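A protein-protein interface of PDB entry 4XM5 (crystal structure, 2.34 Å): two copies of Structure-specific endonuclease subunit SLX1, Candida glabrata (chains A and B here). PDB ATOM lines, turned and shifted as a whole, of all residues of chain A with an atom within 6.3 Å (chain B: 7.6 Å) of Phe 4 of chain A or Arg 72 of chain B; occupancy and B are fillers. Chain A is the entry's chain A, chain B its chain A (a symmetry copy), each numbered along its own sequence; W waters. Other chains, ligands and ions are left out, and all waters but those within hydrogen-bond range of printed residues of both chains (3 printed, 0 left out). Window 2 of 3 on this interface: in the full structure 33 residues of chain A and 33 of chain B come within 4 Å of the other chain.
Of the printed residues of chain B, Glu 2 of chain A touches Tyr 11 (3.9 Å). Phe 4 of chain A touches one residue of chain B. Of the printed residues of chain B, Ile 296 of chain A touches Arg 72 (3.5 Å). Lys 300 of chain A touches none of the printed residues of chain B. Of the printed residues of chain A, Ser 71 of chain B touches Gln 5. Arg 72 of chain B touches just these residues of chain A: Glu 3 (3.0 Å), Phe 4 (3.5 Å), Gln 5 (2.6 Å) and Ile 296 (3.5 Å). Ala 75 of chain B touches none of the printed residues of chain A. The nearest residue of chain B that does not touch Phe 4 of chain A is Tyr 11 of chain B (5.9 Å). The nearest printed residue of chain B that does not touch Glu 2 of chain A is Arg 72 of chain B (4.4 Å).
O of Glu 2 of chain A touches CE2 of Tyr 11 of chain B, at 3.9 Å. Tyr 11 of chain B touches Glu 3 of chain A. Phe 4 of chain A touches Arg 72 of chain B (C to NH1, 3.5 Å). Ser 71 of chain B touches Gln 5 of chain A (CA to OE1, 3.4 Å). Ile 296 of chain A touches Arg 72 of chain B.
Gln 5 of chain A touches its own counterpart, Gln 5 of chain B.
Water W3 lies within hydrogen-bond range of the side-chain amide oxygen (OD1) of Asn 299 of chain A (2.4 Å), the backbone NH (N) of Lys 300 of chain A (2.9 Å), the backbone carbonyl oxygen (O) of Ile 296 of chain A (2.9 Å) and the guanidinium group (NH1) of Arg 72 of chain B (3.2 Å). Water W2 lies within hydrogen-bond range of O of Pro 70 of chain B (2.7 Å), O of Gln 6 of chain B (2.7 Å) and NE2 of Gln 5 of chain A (3.1 Å). Water W1 bridges O of Gln 6 of chain A (2.7 Å) and NE2 of Gln 5 of chain B (3.1 Å).
The guanidinium group (NH1) of Arg 72 of chain B lies close to the backbone carbonyl oxygen (O) of Glu 3 of chain A (3.1 Å). NE2 of Gln 5 of chain B sits close to NE2 of Gln 5 of chain A (2.8 Å). The side-chain amide oxygen of Gln 5 of chain A sits at hydrogen-bond distance from the backbone NH of Arg 72 of chain B (2.6 Å).
Printed residues of chain B that touch a printed residue of chain A: Gln 5, Tyr 11, Ser 71 and Arg 72. Hydrophobic or aromatic side chains of chain B within 4 Å of the printed part of chain A: Tyr 11. Hydrophobic or aromatic side chains of chain A within 4 Å of the printed part of chain B: Ile 296. Among the printed residues, 8 pairs touch across the chains. Among the printed residues, no Asp or Glu carboxylate lies within 4 Å of a Lys or Arg side-chain nitrogen of the other chain.
The backbone NH (N) of Ile 73 of chain B is in hydrogen-bond range of the side-chain hydroxyl (OG) of Ser 71 of chain B (3.0 Å). The side-chain hydroxyl of Ser 71 of chain B lies within hydrogen-bond range of the backbone NH of Ala 74 of chain B.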
ATOM      1  N   GLU A   2       5.102 -12.980 -16.689  1.00  0.00           N
ATOM      2  CA  GLU A   2       4.514 -13.468 -17.931  1.00  0.00           C
ATOM      3  C   GLU A   2       5.504 -14.348 -18.691  1.00  0.00           C
ATOM      4  O   GLU A   2       6.438 -14.913 -18.110  1.00  0.00           O
ATOM      5  CB  GLU A   2       4.063 -12.294 -18.807  1.00  0.00           C
ATOM      6  N   GLU A   3       5.304 -14.452 -19.998  1.00  0.00           N
ATOM      7  CA  GLU A   3       6.194 -15.240 -20.836  1.00  0.00           C
ATOM      8  C   GLU A   3       7.411 -14.427 -21.276  1.00  0.00           C
ATOM      9  O   GLU A   3       8.178 -14.864 -22.133  1.00  0.00           O
ATOM     10  CB  GLU A   3       5.445 -15.763 -22.058  1.00  0.00           C
ATOM     11  CG  GLU A   3       4.929 -14.665 -22.944  1.00  0.00           C
ATOM     12  CD  GLU A   3       4.022 -15.182 -24.030  1.00  0.00           C
ATOM     13  OE1 GLU A   3       4.446 -16.093 -24.775  1.00  0.00           O
ATOM     14  OE2 GLU A   3       2.882 -14.684 -24.137  1.00  0.00           O
ATOM     15  N   PHE A   4       7.599 -13.247 -20.685  1.00  0.00           N
ATOM     16  CA  PHE A   4       8.761 -12.429 -21.015  1.00  0.00           C
ATOM     17  C   PHE A   4       9.683 -12.183 -19.818  1.00  0.00           C
ATOM     18  O   PHE A   4      10.575 -11.325 -19.884  1.00  0.00           O
ATOM     19  CB  PHE A   4       8.309 -11.099 -21.623  1.00  0.00           C
ATOM     20  CG  PHE A   4       7.793 -11.233 -23.026  1.00  0.00           C
ATOM     21  CD1 PHE A   4       8.659 -11.155 -24.108  1.00  0.00           C
ATOM     22  CD2 PHE A   4       6.444 -11.476 -23.265  1.00  0.00           C
ATOM     23  CE1 PHE A   4       8.190 -11.305 -25.400  1.00  0.00           C
ATOM     24  CE2 PHE A   4       5.966 -11.623 -24.555  1.00  0.00           C
ATOM     25  CZ  PHE A   4       6.840 -11.535 -25.626  1.00  0.00           C
ATOM     26  N   GLN A   5       9.480 -12.932 -18.734  1.00  0.00           N
ATOM     27  CA  GLN A   5      10.314 -12.757 -17.542  1.00  0.00           C
ATOM     28  C   GLN A   5      11.734 -13.181 -17.899  1.00  0.00           C
ATOM     29  O   GLN A   5      11.928 -14.132 -18.652  1.00  0.00           O
ATOM     30  CB  GLN A   5       9.749 -13.540 -16.336  1.00  0.00           C
ATOM     31  CG  GLN A   5      10.519 -14.776 -15.877  1.00  0.00           C
ATOM     32  CD  GLN A   5       9.834 -15.516 -14.696  1.00  0.00           C
ATOM     33  OE1 GLN A   5       9.159 -16.540 -14.879  1.00  0.00           O
ATOM     34  NE2 GLN A   5      10.019 -14.994 -13.488  1.00  0.00           N
ATOM     35  N   GLN A   6      12.726 -12.449 -17.398  1.00  0.00           N
ATOM     36  CA  GLN A   6      14.109 -12.712 -17.771  1.00  0.00           C
ATOM     37  C   GLN A   6      14.882 -13.311 -16.618  1.00  0.00           C
ATOM     38  O   GLN A   6      14.466 -13.220 -15.470  1.00  0.00           O
ATOM     39  CB  GLN A   6      14.804 -11.430 -18.262  1.00  0.00           C
ATOM     40  CG  GLN A   6      15.026 -10.341 -17.192  1.00  0.00           C
ATOM     41  CD  GLN A   6      16.109  -9.310 -17.579  1.00  0.00           C
ATOM     42  OE1 GLN A   6      15.801  -8.227 -18.082  1.00  0.00           O
ATOM     43  NE2 GLN A   6      17.376  -9.656 -17.349  1.00  0.00           N
ATOM     44  N   LEU A 238      13.839 -18.011 -30.189  1.00  0.00           N
ATOM     45  CA  LEU A 238      14.975 -17.813 -29.294  1.00  0.00           C
ATOM     46  C   LEU A 238      16.352 -18.191 -29.910  1.00  0.00           C
ATOM     47  O   LEU A 238      16.496 -19.249 -30.528  1.00  0.00           O
ATOM     48  CB  LEU A 238      14.747 -18.612 -28.020  1.00  0.00           C
ATOM     49  CG  LEU A 238      13.567 -18.273 -27.101  1.00  0.00           C
ATOM     50  CD1 LEU A 238      13.485 -19.303 -25.992  1.00  0.00           C
ATOM     51  CD2 LEU A 238      13.689 -16.876 -26.480  1.00  0.00           C
ATOM     52  N   ILE A 296      17.198 -15.146 -23.641  1.00  0.00           N
ATOM     53  CA  ILE A 296      15.936 -14.696 -23.069  1.00  0.00           C
ATOM     54  C   ILE A 296      15.874 -13.183 -23.108  1.00  0.00           C
ATOM     55  O   ILE A 296      14.863 -12.590 -23.475  1.00  0.00           O
ATOM     56  CB  ILE A 296      15.775 -15.186 -21.600  1.00  0.00           C
ATOM     57  CG1 ILE A 296      15.487 -16.689 -21.558  1.00  0.00           C
ATOM     58  CG2 ILE A 296      14.688 -14.419 -20.894  1.00  0.00           C
ATOM     59  CD1 ILE A 296      14.377 -17.146 -22.501  1.00  0.00           C
ATOM     60  N   ASN A 299      15.452 -11.651 -26.536  1.00  0.00           N
ATOM     61  CA  ASN A 299      14.076 -11.831 -26.934  1.00  0.00           C
ATOM     62  C   ASN A 299      13.171 -10.835 -26.226  1.00  0.00           C
ATOM     63  O   ASN A 299      12.321 -10.210 -26.848  1.00  0.00           O
ATOM     64  CB  ASN A 299      13.626 -13.250 -26.640  1.00  0.00           C
ATOM     65  CG  ASN A 299      12.184 -13.473 -26.996  1.00  0.00           C
ATOM     66  OD1 ASN A 299      11.300 -13.337 -26.156  1.00  0.00           O
ATOM     67  ND2 ASN A 299      11.933 -13.796 -28.252  1.00  0.00           N
ATOM     68  N   LYS A 300      13.374 -10.688 -24.920  1.00  0.00           N
ATOM     69  CA  LYS A 300      12.587  -9.776 -24.089  1.00  0.00           C
ATOM     70  C   LYS A 300      12.718  -8.314 -24.502  1.00  0.00           C
ATOM     71  O   LYS A 300      11.717  -7.613 -24.654  1.00  0.00           O
ATOM     72  CB  LYS A 300      12.996  -9.914 -22.621  1.00  0.00           C
ATOM     73  CG  LYS A 300      12.470  -8.793 -21.720  1.00  0.00           C
ATOM     74  CD  LYS A 300      13.121  -8.836 -20.339  1.00  0.00           C
ATOM     75  CE  LYS A 300      12.556  -7.772 -19.413  1.00  0.00           C
ATOM     76  NZ  LYS A 300      13.647  -6.998 -18.725  1.00  0.00           N
ATOM     77  N   ASP A 301      13.955  -7.856 -24.666  1.00  0.00           N
ATOM     78  CA  ASP A 301      14.207  -6.445 -24.935  1.00  0.00           C
ATOM     79  C   ASP A 301      13.569  -5.992 -26.247  1.00  0.00           C
ATOM     80  O   ASP A 301      13.053  -4.878 -26.331  1.00  0.00           O
ATOM     81  CB  ASP A 301      15.714  -6.162 -24.945  1.00  0.00           C
ATOM     82  CG  ASP A 301      16.282  -5.957 -23.542  1.00  0.00           C
ATOM     83  OD1 ASP A 301      15.583  -6.278 -22.543  1.00  0.00           O
ATOM     84  OD2 ASP A 301      17.434  -5.470 -23.443  1.00  0.00           O
ATOM     85  N   THR A 303      10.693  -7.077 -27.868  1.00  0.00           N
ATOM     86  CA  THR A 303       9.279  -6.815 -27.641  1.00  0.00           C
ATOM     87  C   THR A 303       9.073  -5.722 -26.592  1.00  0.00           C
ATOM     88  O   THR A 303       8.278  -4.798 -26.786  1.00  0.00           O
ATOM     89  CB  THR A 303       8.554  -8.085 -27.191  1.00  0.00           C
ATOM     90  OG1 THR A 303       8.999  -8.446 -25.875  1.00  0.00           O
ATOM     91  CG2 THR A 303       8.844  -9.221 -28.160  1.00  0.00           C
ATOM     92  N   GLN B   5       9.925 -10.246  -8.061  1.00  0.00           N
ATOM     93  CA  GLN B   5       9.452 -11.194  -9.073  1.00  0.00           C
ATOM     94  C   GLN B   5       8.770 -12.349  -8.350  1.00  0.00           C
ATOM     95  O   GLN B   5       9.212 -12.761  -7.280  1.00  0.00           O
ATOM     96  CB  GLN B   5      10.604 -11.667  -9.987  1.00  0.00           C
ATOM     97  CG  GLN B   5      11.085 -13.107  -9.826  1.00  0.00           C
ATOM     98  CD  GLN B   5      12.279 -13.458 -10.753  1.00  0.00           C
ATOM     99  OE1 GLN B   5      13.443 -13.482 -10.328  1.00  0.00           O
ATOM    100  NE2 GLN B   5      11.980 -13.736 -12.018  1.00  0.00           N
ATOM    101  N   GLN B   6       7.666 -12.842  -8.906  1.00  0.00           N
ATOM    102  CA  GLN B   6       6.888 -13.873  -8.233  1.00  0.00           C
ATOM    103  C   GLN B   6       7.017 -15.204  -8.937  1.00  0.00           C
ATOM    104  O   GLN B   6       7.418 -15.266 -10.092  1.00  0.00           O
ATOM    105  CB  GLN B   6       5.405 -13.471  -8.133  1.00  0.00           C
ATOM    106  CG  GLN B   6       4.642 -13.402  -9.471  1.00  0.00           C
ATOM    107  CD  GLN B   6       3.108 -13.467  -9.309  1.00  0.00           C
ATOM    108  OE1 GLN B   6       2.429 -12.437  -9.296  1.00  0.00           O
ATOM    109  NE2 GLN B   6       2.569 -14.679  -9.177  1.00  0.00           N
ATOM    110  N   ILE B   7       6.705 -16.276  -8.223  1.00  0.00           N
ATOM    111  CA  ILE B   7       6.402 -17.525  -8.876  1.00  0.00           C
ATOM    112  C   ILE B   7       5.111 -17.339  -9.674  1.00  0.00           C
ATOM    113  O   ILE B   7       4.107 -16.888  -9.126  1.00  0.00           O
ATOM    114  CB  ILE B   7       6.247 -18.674  -7.861  1.00  0.00           C
ATOM    115  CG1 ILE B   7       7.598 -19.001  -7.212  1.00  0.00           C
ATOM    116  CG2 ILE B   7       5.622 -19.919  -8.523  1.00  0.00           C
ATOM    117  CD1 ILE B   7       7.482 -19.714  -5.885  1.00  0.00           C
ATOM    118  N   PRO B   8       5.137 -17.670 -10.978  1.00  0.00           N
ATOM    119  CA  PRO B   8       3.978 -17.498 -11.855  1.00  0.00           C
ATOM    120  C   PRO B   8       2.693 -18.105 -11.285  1.00  0.00           C
ATOM    121  O   PRO B   8       2.737 -19.215 -10.751  1.00  0.00           O
ATOM    122  CB  PRO B   8       4.392 -18.244 -13.132  1.00  0.00           C
ATOM    123  CG  PRO B   8       5.895 -18.202 -13.122  1.00  0.00           C
ATOM    124  CD  PRO B   8       6.253 -18.346 -11.673  1.00  0.00           C
ATOM    125  N   TYR B  11       2.246 -21.782 -14.787  1.00  0.00           N
ATOM    126  CA  TYR B  11       3.223 -21.967 -15.845  1.00  0.00           C
ATOM    127  C   TYR B  11       3.392 -23.457 -16.043  1.00  0.00           C
ATOM    128  O   TYR B  11       3.775 -24.161 -15.123  1.00  0.00           O
ATOM    129  CB  TYR B  11       4.588 -21.271 -15.541  1.00  0.00           C
ATOM    130  CG  TYR B  11       5.157 -20.652 -16.804  1.00  0.00           C
ATOM    131  CD1 TYR B  11       5.609 -21.462 -17.846  1.00  0.00           C
ATOM    132  CD2 TYR B  11       5.158 -19.269 -17.000  1.00  0.00           C
ATOM    133  CE1 TYR B  11       6.075 -20.914 -19.062  1.00  0.00           C
ATOM    134  CE2 TYR B  11       5.622 -18.706 -18.193  1.00  0.00           C
ATOM    135  CZ  TYR B  11       6.079 -19.541 -19.219  1.00  0.00           C
ATOM    136  OH  TYR B  11       6.556 -19.019 -20.393  1.00  0.00           O
ATOM    137  N   CYS B  13       4.218 -27.063 -18.754  1.00  0.00           N
ATOM    138  CA  CYS B  13       4.813 -27.712 -19.922  1.00  0.00           C
ATOM    139  C   CYS B  13       3.873 -28.808 -20.403  1.00  0.00           C
ATOM    140  O   CYS B  13       3.589 -29.736 -19.659  1.00  0.00           O
ATOM    141  CB  CYS B  13       6.175 -28.336 -19.589  1.00  0.00           C
ATOM    142  SG  CYS B  13       7.563 -27.231 -19.555  1.00  0.00           S
ATOM    143  N   SER B  29       5.516 -24.868 -23.846  1.00  0.00           N
ATOM    144  CA  SER B  29       5.244 -24.393 -22.491  1.00  0.00           C
ATOM    145  C   SER B  29       4.670 -22.998 -22.530  1.00  0.00           C
ATOM    146  O   SER B  29       4.901 -22.278 -23.477  1.00  0.00           O
ATOM    147  CB  SER B  29       6.513 -24.440 -21.597  1.00  0.00           C
ATOM    148  OG  SER B  29       7.544 -23.587 -22.052  1.00  0.00           O
ATOM    149  N   THR B  30       3.930 -22.614 -21.486  1.00  0.00           N
ATOM    150  CA  THR B  30       3.066 -21.439 -21.571  1.00  0.00           C
ATOM    151  C   THR B  30       2.486 -21.106 -20.207  1.00  0.00           C
ATOM    152  O   THR B  30       2.310 -21.994 -19.380  1.00  0.00           O
ATOM    153  CB  THR B  30       1.891 -21.677 -22.602  1.00  0.00           C
ATOM    154  OG1 THR B  30       1.133 -20.480 -22.763  1.00  0.00           O
ATOM    155  CG2 THR B  30       0.972 -22.813 -22.145  1.00  0.00           C
ATOM    156  N   PRO B  31       2.215 -19.809 -19.960  1.00  0.00           N
ATOM    157  CA  PRO B  31       1.508 -19.402 -18.741  1.00  0.00           C
ATOM    158  C   PRO B  31      -0.022 -19.441 -18.907  1.00  0.00           C
ATOM    159  O   PRO B  31      -0.736 -19.181 -17.942  1.00  0.00           O
ATOM    160  CB  PRO B  31       1.989 -17.965 -18.527  1.00  0.00           C
ATOM    161  CG  PRO B  31       2.217 -17.446 -19.929  1.00  0.00           C
ATOM    162  CD  PRO B  31       2.688 -18.642 -20.743  1.00  0.00           C
ATOM    163  N   PHE B  69       5.793 -24.585 -11.953  1.00  0.00           N
ATOM    164  CA  PHE B  69       7.209 -24.204 -12.105  1.00  0.00           C
ATOM    165  C   PHE B  69       7.548 -22.872 -11.382  1.00  0.00           C
ATOM    166  O   PHE B  69       6.722 -21.949 -11.367  1.00  0.00           O
ATOM    167  CB  PHE B  69       7.548 -24.125 -13.602  1.00  0.00           C
ATOM    168  CG  PHE B  69       7.639 -25.473 -14.274  1.00  0.00           C
ATOM    169  CD1 PHE B  69       8.794 -26.230 -14.173  1.00  0.00           C
ATOM    170  CD2 PHE B  69       6.545 -25.993 -14.993  1.00  0.00           C
ATOM    171  CE1 PHE B  69       8.889 -27.464 -14.779  1.00  0.00           C
ATOM    172  CE2 PHE B  69       6.625 -27.253 -15.610  1.00  0.00           C
ATOM    173  CZ  PHE B  69       7.797 -27.989 -15.500  1.00  0.00           C
ATOM    174  N   PRO B  70       8.735 -22.780 -10.748  1.00  0.00           N
ATOM    175  CA  PRO B  70       8.999 -21.552  -9.974  1.00  0.00           C
ATOM    176  C   PRO B  70       9.153 -20.318 -10.865  1.00  0.00           C
ATOM    177  O   PRO B  70       9.122 -19.195 -10.357  1.00  0.00           O
ATOM    178  CB  PRO B  70      10.323 -21.853  -9.237  1.00  0.00           C
ATOM    179  CG  PRO B  70      10.994 -22.990 -10.053  1.00  0.00           C
ATOM    180  CD  PRO B  70       9.769 -23.815 -10.533  1.00  0.00           C
ATOM    181  N   SER B  71       9.307 -20.529 -12.174  1.00  0.00           N
ATOM    182  CA  SER B  71       9.524 -19.436 -13.136  1.00  0.00           C
ATOM    183  C   SER B  71       9.421 -19.967 -14.555  1.00  0.00           C
ATOM    184  O   SER B  71       9.437 -21.189 -14.783  1.00  0.00           O
ATOM    185  CB  SER B  71      10.910 -18.789 -12.948  1.00  0.00           C
ATOM    186  OG  SER B  71      11.909 -19.564 -13.610  1.00  0.00           O
ATOM    187  N   ARG B  72       9.347 -19.036 -15.496  1.00  0.00           N
ATOM    188  CA  ARG B  72       9.503 -19.328 -16.907  1.00  0.00           C
ATOM    189  C   ARG B  72      10.786 -20.114 -17.227  1.00  0.00           C
ATOM    190  O   ARG B  72      10.766 -21.032 -18.039  1.00  0.00           O
ATOM    191  CB  ARG B  72       9.509 -18.019 -17.702  1.00  0.00           C
ATOM    192  CG  ARG B  72       9.616 -18.194 -19.210  1.00  0.00           C
ATOM    193  CD  ARG B  72      10.091 -16.898 -19.829  1.00  0.00           C
ATOM    194  NE  ARG B  72      10.358 -17.007 -21.262  1.00  0.00           N
ATOM    195  CZ  ARG B  72      10.894 -16.033 -21.994  1.00  0.00           C
ATOM    196  NH1 ARG B  72      11.223 -14.877 -21.425  1.00  0.00           N
ATOM    197  NH2 ARG B  72      11.100 -16.214 -23.293  1.00  0.00           N
ATOM    198  N   ILE B  73      11.902 -19.741 -16.614  1.00  0.00           N
ATOM    199  CA  ILE B  73      13.176 -20.347 -16.979  1.00  0.00           C
ATOM    200  C   ILE B  73      13.169 -21.842 -16.688  1.00  0.00           C
ATOM    201  O   ILE B  73      13.569 -22.650 -17.531  1.00  0.00           O
ATOM    202  CB  ILE B  73      14.366 -19.685 -16.240  1.00  0.00           C
ATOM    203  CG1 ILE B  73      14.313 -18.172 -16.407  1.00  0.00           C
ATOM    204  CG2 ILE B  73      15.698 -20.223 -16.754  1.00  0.00           C
ATOM    205  CD1 ILE B  73      14.170 -17.708 -17.854  1.00  0.00           C
ATOM    206  N   ALA B  74      12.710 -22.212 -15.500  1.00  0.00           N
ATOM    207  CA  ALA B  74      12.679 -23.606 -15.141  1.00  0.00           C
ATOM    208  C   ALA B  74      11.685 -24.394 -16.037  1.00  0.00           C
ATOM    209  O   ALA B  74      11.955 -25.543 -16.399  1.00  0.00           O
ATOM    210  CB  ALA B  74      12.350 -23.741 -13.699  1.00  0.00           C
ATOM    211  N   ALA B  75      10.573 -23.785 -16.431  1.00  0.00           N
ATOM    212  CA  ALA B  75       9.658 -24.444 -17.388  1.00  0.00           C
ATOM    213  C   ALA B  75      10.317 -24.650 -18.755  1.00  0.00           C
ATOM    214  O   ALA B  75      10.208 -25.715 -19.347  1.00  0.00           O
ATOM    215  CB  ALA B  75       8.387 -23.662 -17.548  1.00  0.00           C
ATOM    216  N   LEU B  76      11.024 -23.634 -19.238  1.00  0.00           N
ATOM    217  CA  LEU B  76      11.790 -23.747 -20.474  1.00  0.00           C
ATOM    218  C   LEU B  76      12.755 -24.936 -20.448  1.00  0.00           C
ATOM    219  O   LEU B  76      12.843 -25.702 -21.412  1.00  0.00           O
ATOM    220  CB  LEU B  76      12.574 -22.460 -20.728  1.00  0.00           C
ATOM    221  CG  LEU B  76      13.332 -22.393 -22.058  1.00  0.00           C
ATOM    222  CD1 LEU B  76      12.363 -22.429 -23.240  1.00  0.00           C
ATOM    223  CD2 LEU B  76      14.207 -21.147 -22.114  1.00  0.00           C
ATOM    224  N   GLN B  77      13.485 -25.096 -19.355  1.00  0.00           N
ATOM    225  CA  GLN B  77      14.431 -26.190 -19.300  1.00  0.00           C
ATOM    226  C   GLN B  77      13.794 -27.586 -19.176  1.00  0.00           C
ATOM    227  O   GLN B  77      14.349 -28.565 -19.675  1.00  0.00           O
ATOM    228  CB  GLN B  77      15.394 -25.933 -18.165  1.00  0.00           C
ATOM    229  CG  GLN B  77      16.181 -24.650 -18.432  1.00  0.00           C
ATOM    230  CD  GLN B  77      17.351 -24.513 -17.533  1.00  0.00           C
ATOM    231  OE1 GLN B  77      17.239 -23.954 -16.457  1.00  0.00           O
ATOM    232  NE2 GLN B  77      18.491 -25.040 -17.956  1.00  0.00           N
ATOM    233  N   PHE B  78      12.639 -27.668 -18.511  1.00  0.00           N
ATOM    234  CA  PHE B  78      11.852 -28.893 -18.471  1.00  0.00           C
ATOM    235  C   PHE B  78      11.469 -29.218 -19.915  1.00  0.00           C
ATOM    236  O   PHE B  78      11.674 -30.332 -20.388  1.00  0.00           O
ATOM    237  CB  PHE B  78      10.612 -28.719 -17.581  1.00  0.00           C
ATOM    238  CG  PHE B  78       9.903 -30.006 -17.241  1.00  0.00           C
ATOM    239  CD1 PHE B  78       8.891 -30.495 -18.055  1.00  0.00           C
ATOM    240  CD2 PHE B  78      10.241 -30.717 -16.091  1.00  0.00           C
ATOM    241  CE1 PHE B  78       8.219 -31.671 -17.721  1.00  0.00           C
ATOM    242  CE2 PHE B  78       9.595 -31.882 -15.748  1.00  0.00           C
ATOM    243  CZ  PHE B  78       8.581 -32.372 -16.563  1.00  0.00           C
ATOM    244  N   GLN B  79      10.953 -28.212 -20.612  1.00  0.00           N
ATOM    245  CA  GLN B  79      10.633 -28.324 -22.035  1.00  0.00           C
ATOM    246  C   GLN B  79      11.804 -28.805 -22.899  1.00  0.00           C
ATOM    247  O   GLN B  79      11.661 -29.767 -23.658  1.00  0.00           O
ATOM    248  CB  GLN B  79      10.155 -26.981 -22.564  1.00  0.00           C
ATOM    249  CG  GLN B  79       9.749 -26.993 -24.015  1.00  0.00           C
ATOM    250  CD  GLN B  79       9.766 -25.595 -24.595  1.00  0.00           C
ATOM    251  OE1 GLN B  79       9.090 -24.681 -24.097  1.00  0.00           O
ATOM    252  NE2 GLN B  79      10.565 -25.405 -25.631  1.00  0.00           N
HETATM  253  O   HOH W   1      13.808 -15.382 -13.943  1.00  0.00           O
HETATM  254  O   HOH W   2       9.699 -16.576 -10.814  1.00  0.00           O
HETATM  255  O   HOH W   3      11.996 -13.018 -23.855  1.00  0.00           O
